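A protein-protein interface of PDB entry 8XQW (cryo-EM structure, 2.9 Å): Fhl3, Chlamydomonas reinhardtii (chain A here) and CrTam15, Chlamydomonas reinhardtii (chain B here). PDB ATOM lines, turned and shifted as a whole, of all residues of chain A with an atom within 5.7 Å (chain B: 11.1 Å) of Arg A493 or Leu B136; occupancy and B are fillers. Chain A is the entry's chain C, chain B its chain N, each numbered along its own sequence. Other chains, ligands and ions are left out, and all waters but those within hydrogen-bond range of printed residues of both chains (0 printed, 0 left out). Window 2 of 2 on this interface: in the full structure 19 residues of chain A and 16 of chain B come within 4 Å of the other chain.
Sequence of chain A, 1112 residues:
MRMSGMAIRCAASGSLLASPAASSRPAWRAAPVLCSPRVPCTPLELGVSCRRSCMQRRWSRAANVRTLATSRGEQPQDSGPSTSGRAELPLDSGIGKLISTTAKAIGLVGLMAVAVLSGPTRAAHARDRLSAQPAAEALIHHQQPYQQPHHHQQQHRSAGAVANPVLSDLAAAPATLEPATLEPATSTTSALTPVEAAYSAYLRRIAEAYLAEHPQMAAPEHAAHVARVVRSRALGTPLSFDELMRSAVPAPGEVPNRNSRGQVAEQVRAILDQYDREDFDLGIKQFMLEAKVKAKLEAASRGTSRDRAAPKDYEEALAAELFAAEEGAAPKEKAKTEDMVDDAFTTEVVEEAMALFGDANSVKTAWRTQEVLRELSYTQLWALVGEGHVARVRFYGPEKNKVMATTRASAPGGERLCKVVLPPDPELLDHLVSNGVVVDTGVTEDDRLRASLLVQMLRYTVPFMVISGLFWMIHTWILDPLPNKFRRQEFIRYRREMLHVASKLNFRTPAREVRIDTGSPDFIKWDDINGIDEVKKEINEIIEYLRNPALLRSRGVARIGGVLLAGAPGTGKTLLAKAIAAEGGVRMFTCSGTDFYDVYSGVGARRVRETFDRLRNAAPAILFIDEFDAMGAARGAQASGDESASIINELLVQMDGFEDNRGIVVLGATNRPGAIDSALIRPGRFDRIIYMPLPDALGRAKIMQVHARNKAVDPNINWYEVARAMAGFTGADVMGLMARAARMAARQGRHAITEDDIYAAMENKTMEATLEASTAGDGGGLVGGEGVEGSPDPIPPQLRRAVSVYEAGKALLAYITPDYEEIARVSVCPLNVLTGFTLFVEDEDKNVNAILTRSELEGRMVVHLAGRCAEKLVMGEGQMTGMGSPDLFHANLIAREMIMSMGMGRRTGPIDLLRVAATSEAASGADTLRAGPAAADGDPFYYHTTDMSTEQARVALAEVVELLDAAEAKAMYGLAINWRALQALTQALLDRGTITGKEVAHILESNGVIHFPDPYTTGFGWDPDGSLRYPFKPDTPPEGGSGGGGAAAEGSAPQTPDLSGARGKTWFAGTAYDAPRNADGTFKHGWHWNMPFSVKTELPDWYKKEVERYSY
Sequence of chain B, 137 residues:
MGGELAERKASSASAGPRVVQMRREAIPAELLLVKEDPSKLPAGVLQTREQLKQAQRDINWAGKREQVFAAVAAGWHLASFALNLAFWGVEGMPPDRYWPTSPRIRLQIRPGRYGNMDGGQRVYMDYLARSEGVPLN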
ATOM      1  N   ARG A 488      11.228  30.565  37.539  1.00  0.00           N
ATOM      2  CA  ARG A 488      11.656  30.928  36.193  1.00  0.00           C
ATOM      3  C   ARG A 488      11.157  29.920  35.170  1.00  0.00           C
ATOM      4  O   ARG A 488      10.660  30.294  34.101  1.00  0.00           O
ATOM      5  CB  ARG A 488      13.176  31.039  36.137  1.00  0.00           C
ATOM      6  CG  ARG A 488      13.685  32.459  36.147  1.00  0.00           C
ATOM      7  CD  ARG A 488      15.188  32.502  36.023  1.00  0.00           C
ATOM      8  NE  ARG A 488      15.831  32.142  37.276  1.00  0.00           N
ATOM      9  CZ  ARG A 488      16.815  31.260  37.379  1.00  0.00           C
ATOM     10  NH1 ARG A 488      17.282  30.654  36.300  1.00  0.00           N
ATOM     11  NH2 ARG A 488      17.334  30.986  38.564  1.00  0.00           N
ATOM     12  N   GLN A 489      11.287  28.628  35.481  1.00  0.00           N
ATOM     13  CA  GLN A 489      10.797  27.596  34.574  1.00  0.00           C
ATOM     14  C   GLN A 489       9.299  27.726  34.351  1.00  0.00           C
ATOM     15  O   GLN A 489       8.825  27.683  33.205  1.00  0.00           O
ATOM     16  CB  GLN A 489      11.127  26.214  35.127  1.00  0.00           C
ATOM     17  CG  GLN A 489      12.598  25.902  35.158  1.00  0.00           C
ATOM     18  CD  GLN A 489      12.862  24.460  35.501  1.00  0.00           C
ATOM     19  OE1 GLN A 489      11.934  23.658  35.595  1.00  0.00           O
ATOM     20  NE2 GLN A 489      14.128  24.116  35.691  1.00  0.00           N
ATOM     21  N   GLU A 490       8.538  27.879  35.434  1.00  0.00           N
ATOM     22  CA  GLU A 490       7.091  27.999  35.285  1.00  0.00           C
ATOM     23  C   GLU A 490       6.726  29.239  34.480  1.00  0.00           C
ATOM     24  O   GLU A 490       5.787  29.211  33.678  1.00  0.00           O
ATOM     25  CB  GLU A 490       6.418  28.023  36.655  1.00  0.00           C
ATOM     26  CG  GLU A 490       4.908  27.813  36.619  1.00  0.00           C
ATOM     27  CD  GLU A 490       4.126  29.069  36.268  1.00  0.00           C
ATOM     28  OE1 GLU A 490       2.916  28.958  35.973  1.00  0.00           O
ATOM     29  OE2 GLU A 490       4.711  30.171  36.308  1.00  0.00           O
ATOM     30  N   PHE A 491       7.459  30.334  34.678  1.00  0.00           N
ATOM     31  CA  PHE A 491       7.192  31.552  33.927  1.00  0.00           C
ATOM     32  C   PHE A 491       7.413  31.332  32.440  1.00  0.00           C
ATOM     33  O   PHE A 491       6.582  31.724  31.615  1.00  0.00           O
ATOM     34  CB  PHE A 491       8.081  32.681  34.444  1.00  0.00           C
ATOM     35  CG  PHE A 491       7.931  33.964  33.689  1.00  0.00           C
ATOM     36  CD1 PHE A 491       8.651  34.198  32.534  1.00  0.00           C
ATOM     37  CD2 PHE A 491       7.078  34.946  34.146  1.00  0.00           C
ATOM     38  CE1 PHE A 491       8.510  35.376  31.844  1.00  0.00           C
ATOM     39  CE2 PHE A 491       6.937  36.128  33.462  1.00  0.00           C
ATOM     40  CZ  PHE A 491       7.652  36.344  32.311  1.00  0.00           C
ATOM     41  N   ILE A 492       8.547  30.730  32.080  1.00  0.00           N
ATOM     42  CA  ILE A 492       8.829  30.474  30.669  1.00  0.00           C
ATOM     43  C   ILE A 492       7.727  29.625  30.057  1.00  0.00           C
ATOM     44  O   ILE A 492       7.192  29.944  28.983  1.00  0.00           O
ATOM     45  CB  ILE A 492      10.200  29.795  30.512  1.00  0.00           C
ATOM     46  CG1 ILE A 492      11.313  30.703  31.022  1.00  0.00           C
ATOM     47  CG2 ILE A 492      10.441  29.446  29.067  1.00  0.00           C
ATOM     48  CD1 ILE A 492      11.231  32.103  30.500  1.00  0.00           C
ATOM     49  N   ARG A 493       7.379  28.528  30.729  1.00  0.00           N
ATOM     50  CA  ARG A 493       6.335  27.633  30.244  1.00  0.00           C
ATOM     51  C   ARG A 493       5.028  28.381  30.007  1.00  0.00           C
ATOM     52  O   ARG A 493       4.453  28.334  28.908  1.00  0.00           O
ATOM     53  CB  ARG A 493       6.145  26.508  31.259  1.00  0.00           C
ATOM     54  CG  ARG A 493       5.050  25.533  30.953  1.00  0.00           C
ATOM     55  CD  ARG A 493       5.173  24.329  31.864  1.00  0.00           C
ATOM     56  NE  ARG A 493       6.470  23.676  31.718  1.00  0.00           N
ATOM     57  CZ  ARG A 493       7.336  23.493  32.710  1.00  0.00           C
ATOM     58  NH1 ARG A 493       7.050  23.915  33.934  1.00  0.00           N
ATOM     59  NH2 ARG A 493       8.492  22.887  32.479  1.00  0.00           N
ATOM     60  N   TYR A 494       4.550  29.083  31.035  1.00  0.00           N
ATOM     61  CA  TYR A 494       3.279  29.785  30.938  1.00  0.00           C
ATOM     62  C   TYR A 494       3.308  30.841  29.845  1.00  0.00           C
ATOM     63  O   TYR A 494       2.324  31.011  29.123  1.00  0.00           O
ATOM     64  CB  TYR A 494       2.929  30.416  32.286  1.00  0.00           C
ATOM     65  CG  TYR A 494       1.799  31.417  32.226  1.00  0.00           C
ATOM     66  CD1 TYR A 494       0.482  31.017  32.398  1.00  0.00           C
ATOM     67  CD2 TYR A 494       2.048  32.765  32.006  1.00  0.00           C
ATOM     68  CE1 TYR A 494      -0.553  31.928  32.344  1.00  0.00           C
ATOM     69  CE2 TYR A 494       1.020  33.681  31.944  1.00  0.00           C
ATOM     70  CZ  TYR A 494      -0.277  33.258  32.116  1.00  0.00           C
ATOM     71  OH  TYR A 494      -1.301  34.173  32.061  1.00  0.00           O
ATOM     72  N   ARG A 495       4.421  31.558  29.699  1.00  0.00           N
ATOM     73  CA  ARG A 495       4.456  32.656  28.741  1.00  0.00           C
ATOM     74  C   ARG A 495       4.482  32.152  27.308  1.00  0.00           C
ATOM     75  O   ARG A 495       3.847  32.746  26.427  1.00  0.00           O
ATOM     76  CB  ARG A 495       5.660  33.551  29.011  1.00  0.00           C
ATOM     77  CG  ARG A 495       5.305  34.832  29.718  1.00  0.00           C
ATOM     78  CD  ARG A 495       4.172  35.547  29.013  1.00  0.00           C
ATOM     79  NE  ARG A 495       4.073  36.934  29.446  1.00  0.00           N
ATOM     80  CZ  ARG A 495       4.672  37.949  28.834  1.00  0.00           C
ATOM     81  NH1 ARG A 495       5.410  37.729  27.758  1.00  0.00           N
ATOM     82  NH2 ARG A 495       4.531  39.182  29.300  1.00  0.00           N
ATOM     83  N   ARG A 496       5.205  31.059  27.051  1.00  0.00           N
ATOM     84  CA  ARG A 496       5.134  30.455  25.726  1.00  0.00           C
ATOM     85  C   ARG A 496       3.719  29.976  25.423  1.00  0.00           C
ATOM     86  O   ARG A 496       3.144  30.323  24.379  1.00  0.00           O
ATOM     87  CB  ARG A 496       6.125  29.300  25.615  1.00  0.00           C
ATOM     88  CG  ARG A 496       7.564  29.739  25.519  1.00  0.00           C
ATOM     89  CD  ARG A 496       8.477  28.569  25.226  1.00  0.00           C
ATOM     90  NE  ARG A 496       8.331  28.095  23.855  1.00  0.00           N
ATOM     91  CZ  ARG A 496       7.874  26.892  23.528  1.00  0.00           C
ATOM     92  NH1 ARG A 496       7.773  26.546  22.254  1.00  0.00           N
ATOM     93  NH2 ARG A 496       7.518  26.035  24.474  1.00  0.00           N
ATOM     94  N   GLU A 497       3.130  29.204  26.342  1.00  0.00           N
ATOM     95  CA  GLU A 497       1.793  28.673  26.090  1.00  0.00           C
ATOM     96  C   GLU A 497       0.761  29.787  25.990  1.00  0.00           C
ATOM     97  O   GLU A 497      -0.298  29.604  25.377  1.00  0.00           O
ATOM     98  CB  GLU A 497       1.407  27.679  27.182  1.00  0.00           C
ATOM     99  CG  GLU A 497       1.895  26.270  26.918  1.00  0.00           C
ATOM    100  CD  GLU A 497       1.429  25.288  27.967  1.00  0.00           C
ATOM    101  OE1 GLU A 497       0.587  25.669  28.806  1.00  0.00           O
ATOM    102  OE2 GLU A 497       1.905  24.133  27.952  1.00  0.00           O
ATOM    103  N   MET A 498       1.045  30.946  26.580  1.00  0.00           N
ATOM    104  CA  MET A 498       0.134  32.076  26.504  1.00  0.00           C
ATOM    105  C   MET A 498       0.237  32.828  25.192  1.00  0.00           C
ATOM    106  O   MET A 498      -0.779  32.982  24.507  1.00  0.00           O
ATOM    107  CB  MET A 498       0.390  33.049  27.660  1.00  0.00           C
ATOM    108  CG  MET A 498      -0.562  34.241  27.704  1.00  0.00           C
ATOM    109  SD  MET A 498      -0.035  35.668  26.730  1.00  0.00           S
ATOM    110  CE  MET A 498       0.547  36.763  28.019  1.00  0.00           C
ATOM    111  N   MET B 125      11.852  33.514  22.453  1.00  0.00           N
ATOM    112  CA  MET B 125      11.325  32.745  23.569  1.00  0.00           C
ATOM    113  C   MET B 125      11.958  31.365  23.637  1.00  0.00           C
ATOM    114  O   MET B 125      12.407  30.936  24.705  1.00  0.00           O
ATOM    115  CB  MET B 125       9.808  32.640  23.461  1.00  0.00           C
ATOM    116  CG  MET B 125       9.091  33.963  23.626  1.00  0.00           C
ATOM    117  SD  MET B 125       9.526  34.822  25.147  1.00  0.00           S
ATOM    118  CE  MET B 125       9.208  33.557  26.367  1.00  0.00           C
ATOM    119  N   ASP B 126      12.048  30.667  22.500  1.00  0.00           N
ATOM    120  CA  ASP B 126      12.546  29.300  22.600  1.00  0.00           C
ATOM    121  C   ASP B 126      14.010  29.285  23.008  1.00  0.00           C
ATOM    122  O   ASP B 126      14.413  28.429  23.806  1.00  0.00           O
ATOM    123  CB  ASP B 126      12.325  28.522  21.301  1.00  0.00           C
ATOM    124  CG  ASP B 126      13.270  28.926  20.193  1.00  0.00           C
ATOM    125  OD1 ASP B 126      14.454  28.528  20.232  1.00  0.00           O
ATOM    126  OD2 ASP B 126      12.823  29.623  19.266  1.00  0.00           O
ATOM    127  N   TYR B 127      14.801  30.250  22.527  1.00  0.00           N
ATOM    128  CA  TYR B 127      16.155  30.399  23.046  1.00  0.00           C
ATOM    129  C   TYR B 127      16.123  30.491  24.561  1.00  0.00           C
ATOM    130  O   TYR B 127      16.797  29.726  25.258  1.00  0.00           O
ATOM    131  CB  TYR B 127      16.819  31.638  22.454  1.00  0.00           C
ATOM    132  CG  TYR B 127      17.588  31.394  21.184  1.00  0.00           C
ATOM    133  CD1 TYR B 127      16.952  31.386  19.957  1.00  0.00           C
ATOM    134  CD2 TYR B 127      18.957  31.195  21.210  1.00  0.00           C
ATOM    135  CE1 TYR B 127      17.648  31.171  18.798  1.00  0.00           C
ATOM    136  CE2 TYR B 127      19.665  30.979  20.053  1.00  0.00           C
ATOM    137  CZ  TYR B 127      19.004  30.968  18.847  1.00  0.00           C
ATOM    138  OH  TYR B 127      19.704  30.755  17.683  1.00  0.00           O
ATOM    139  N   LEU B 128      15.301  31.401  25.084  1.00  0.00           N
ATOM    140  CA  LEU B 128      15.106  31.497  26.523  1.00  0.00           C
ATOM    141  C   LEU B 128      14.724  30.143  27.100  1.00  0.00           C
ATOM    142  O   LEU B 128      15.357  29.656  28.042  1.00  0.00           O
ATOM    143  CB  LEU B 128      14.036  32.542  26.833  1.00  0.00           C
ATOM    144  CG  LEU B 128      14.003  33.121  28.242  1.00  0.00           C
ATOM    145  CD1 LEU B 128      15.405  33.357  28.738  1.00  0.00           C
ATOM    146  CD2 LEU B 128      13.223  34.411  28.256  1.00  0.00           C
ATOM    147  N   ALA B 129      13.722  29.496  26.506  1.00  0.00           N
ATOM    148  CA  ALA B 129      13.277  28.215  27.032  1.00  0.00           C
ATOM    149  C   ALA B 129      14.395  27.190  27.034  1.00  0.00           C
ATOM    150  O   ALA B 129      14.407  26.299  27.888  1.00  0.00           O
ATOM    151  CB  ALA B 129      12.088  27.698  26.223  1.00  0.00           C
ATOM    152  N   ARG B 130      15.395  27.342  26.176  1.00  0.00           N
ATOM    153  CA  ARG B 130      16.438  26.287  26.120  1.00  0.00           C
ATOM    154  C   ARG B 130      17.575  26.660  27.076  1.00  0.00           C
ATOM    155  O   ARG B 130      18.353  25.768  27.447  1.00  0.00           O
ATOM    156  CB  ARG B 130      16.914  26.094  24.678  1.00  0.00           C
ATOM    157  CG  ARG B 130      15.855  25.490  23.766  1.00  0.00           C
ATOM    158  CD  ARG B 130      16.426  24.919  22.478  1.00  0.00           C
ATOM    159  NE  ARG B 130      17.888  24.813  22.512  1.00  0.00           N
ATOM    160  CZ  ARG B 130      18.577  23.716  22.218  1.00  0.00           C
ATOM    161  NH1 ARG B 130      18.581  22.694  23.055  1.00  0.00           N
ATOM    162  NH2 ARG B 130      19.263  23.649  21.090  1.00  0.00           N
ATOM    163  N   SER B 131      17.646  27.927  27.471  1.00  0.00           N
ATOM    164  CA  SER B 131      18.727  28.403  28.369  1.00  0.00           C
ATOM    165  C   SER B 131      18.348  28.128  29.823  1.00  0.00           C
ATOM    166  O   SER B 131      19.239  27.762  30.603  1.00  0.00           O
ATOM    167  CB  SER B 131      18.966  29.871  28.169  1.00  0.00           C
ATOM    168  OG  SER B 131      18.271  30.640  29.141  1.00  0.00           O
ATOM    169  N   GLU B 132      17.077  28.317  30.161  1.00  0.00           N
ATOM    170  CA  GLU B 132      16.614  28.134  31.556  1.00  0.00           C
ATOM    171  C   GLU B 132      16.413  26.639  31.821  1.00  0.00           C
ATOM    172  O   GLU B 132      16.095  26.279  32.965  1.00  0.00           O
ATOM    173  CB  GLU B 132      15.335  28.950  31.727  1.00  0.00           C
ATOM    174  CG  GLU B 132      15.322  29.803  32.989  1.00  0.00           C
ATOM    175  CD  GLU B 132      15.435  28.950  34.236  1.00  0.00           C
ATOM    176  OE1 GLU B 132      16.551  28.853  34.777  1.00  0.00           O
ATOM    177  OE2 GLU B 132      14.418  28.368  34.654  1.00  0.00           O
ATOM    178  N   GLY B 133      16.583  25.805  30.799  1.00  0.00           N
ATOM    179  CA  GLY B 133      16.472  24.350  30.993  1.00  0.00           C
ATOM    180  C   GLY B 133      15.093  23.832  30.639  1.00  0.00           C
ATOM    181  O   GLY B 133      14.942  22.600  30.559  1.00  0.00           O
ATOM    182  N   VAL B 134      14.113  24.722  30.449  1.00  0.00           N
ATOM    183  CA  VAL B 134      12.715  24.263  30.183  1.00  0.00           C
ATOM    184  C   VAL B 134      12.778  23.250  29.034  1.00  0.00           C
ATOM    185  O   VAL B 134      13.206  23.629  27.929  1.00  0.00           O
ATOM    186  CB  VAL B 134      11.735  25.409  29.877  1.00  0.00           C
ATOM    187  CG1 VAL B 134      10.348  24.893  29.515  1.00  0.00           C
ATOM    188  CG2 VAL B 134      11.653  26.386  31.043  1.00  0.00           C
ATOM    189  N   PRO B 135      12.378  21.981  29.249  1.00  0.00           N
ATOM    190  CA  PRO B 135      12.526  20.965  28.217  1.00  0.00           C
ATOM    191  C   PRO B 135      11.400  20.951  27.201  1.00  0.00           C
ATOM    192  O   PRO B 135      11.502  20.241  26.181  1.00  0.00           O
ATOM    193  CB  PRO B 135      12.538  19.704  29.094  1.00  0.00           C
ATOM    194  CG  PRO B 135      11.551  20.020  30.193  1.00  0.00           C
ATOM    195  CD  PRO B 135      11.776  21.493  30.481  1.00  0.00           C
ATOM    196  N   LEU B 136      10.355  21.732  27.453  1.00  0.00           N
ATOM    197  CA  LEU B 136       9.172  21.705  26.561  1.00  0.00           C
ATOM    198  C   LEU B 136       9.554  22.108  25.132  1.00  0.00           C
ATOM    199  O   LEU B 136       9.205  21.343  24.202  1.00  0.00           O
ATOM    200  CB  LEU B 136       8.139  22.660  27.148  1.00  0.00           C
ATOM    201  CG  LEU B 136       7.012  22.020  27.962  1.00  0.00           C
ATOM    202  CD1 LEU B 136       7.543  21.416  29.251  1.00  0.00           C
ATOM    203  CD2 LEU B 136       5.942  23.055  28.254  1.00  0.00           C
ATOM    204  N   ASN B 137      10.219  23.255  24.957  1.00  0.00           N
ATOM    205  CA  ASN B 137      10.505  23.783  23.625  1.00  0.00           C
ATOM    206  C   ASN B 137       9.227  23.888  22.794  1.00  0.00           C
ATOM    207  O   ASN B 137       9.271  24.113  21.587  1.00  0.00           O
ATOM    208  CB  ASN B 137      11.541  22.918  22.903  1.00  0.00           C
ATOM    209  CG  ASN B 137      12.201  23.645  21.749  1.00  0.00           C
ATOM    210  OD1 ASN B 137      12.018  24.849  21.575  1.00  0.00           O
ATOM    211  ND2 ASN B 137      12.970  22.915  20.951  1.00  0.00           N
ATOM    212  OXT ASN B 137       8.114  23.760  23.305  1.00  0.00           O
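Hydrophobic or aromatic side chains of chain B within 4 Å of the printed part of chain A: Leu B128, Ala B129, Val B134 and Leu B136.
Of the 11 printed residues of chain A, 5 touch a printed residue of chain B.
Hydrophobic or aromatic side chains of chain A within 4 Å of the printed part of chain B: Ile A492.
Among the printed residues, Asp or Glu carboxylates within 4 Å of a Lys or Arg side-chain nitrogen of the other chain: Arg A488 with Glu B132 (2.5 Å).
The side-chain carboxylate of Glu B132 lies close to the backbone NH of Gln A489, at 3.2 Å.
The guanidinium group of Arg A496 is in salt-bridge range of the chain-end carboxylate of Asn B137 (2.6 Å).
The guanidinium group (NH1) of Arg A488 is in salt-bridge range of the side-chain carboxylate (OE1) of Glu B132.
Val B134 touches Gln A489.
CD1 of Ile A492 touches CG of Leu B128, 3.7 Å away.
CG2 of Ile A492 touches CA of Ala B129, 3.7 Å away.
CB of Ile A492 touches CG2 of Val B134 (3.7 Å).
NE of Arg A493 touches CD1 of Leu B136 (3.5 Å).
Ala B129 touches Arg A496.
O of Ala B129 sits at hydrogen-bond distance from N of Val B134.
OG of Ser B131 is in hydrogen-bond range of O of Leu B128 (3.3 Å).
Of the printed residues of chain B, Arg A488 touches Glu B132.
Of the printed residues of chain B, Gln A489 touches Glu B132 and Val B134.
Arg A493 touches just one residue of chain B: Leu B136 (3.5 Å).
Tyr A494 touches none of the printed residues of chain B.
Arg A496 touches just these residues of chain B: Ala B129 (3.8 Å) and Asn B137 (2.6 Å).
Of the printed residues of chain A, Glu B132 touches Arg A488 and Gln A489.
Of chain A, only Arg A493 (3.5 Å) comes within 4 Å of Leu B136.
The nearest residue of chain B that does not touch Arg A493 is Val B134 (4.03 Å).
The nearest residue of chain A that does not touch Leu B136 is Glu A497 (4.2 Å).
The nearest printed residue of chain A that does not touch Leu B128 is Phe A491 (6.0 Å).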
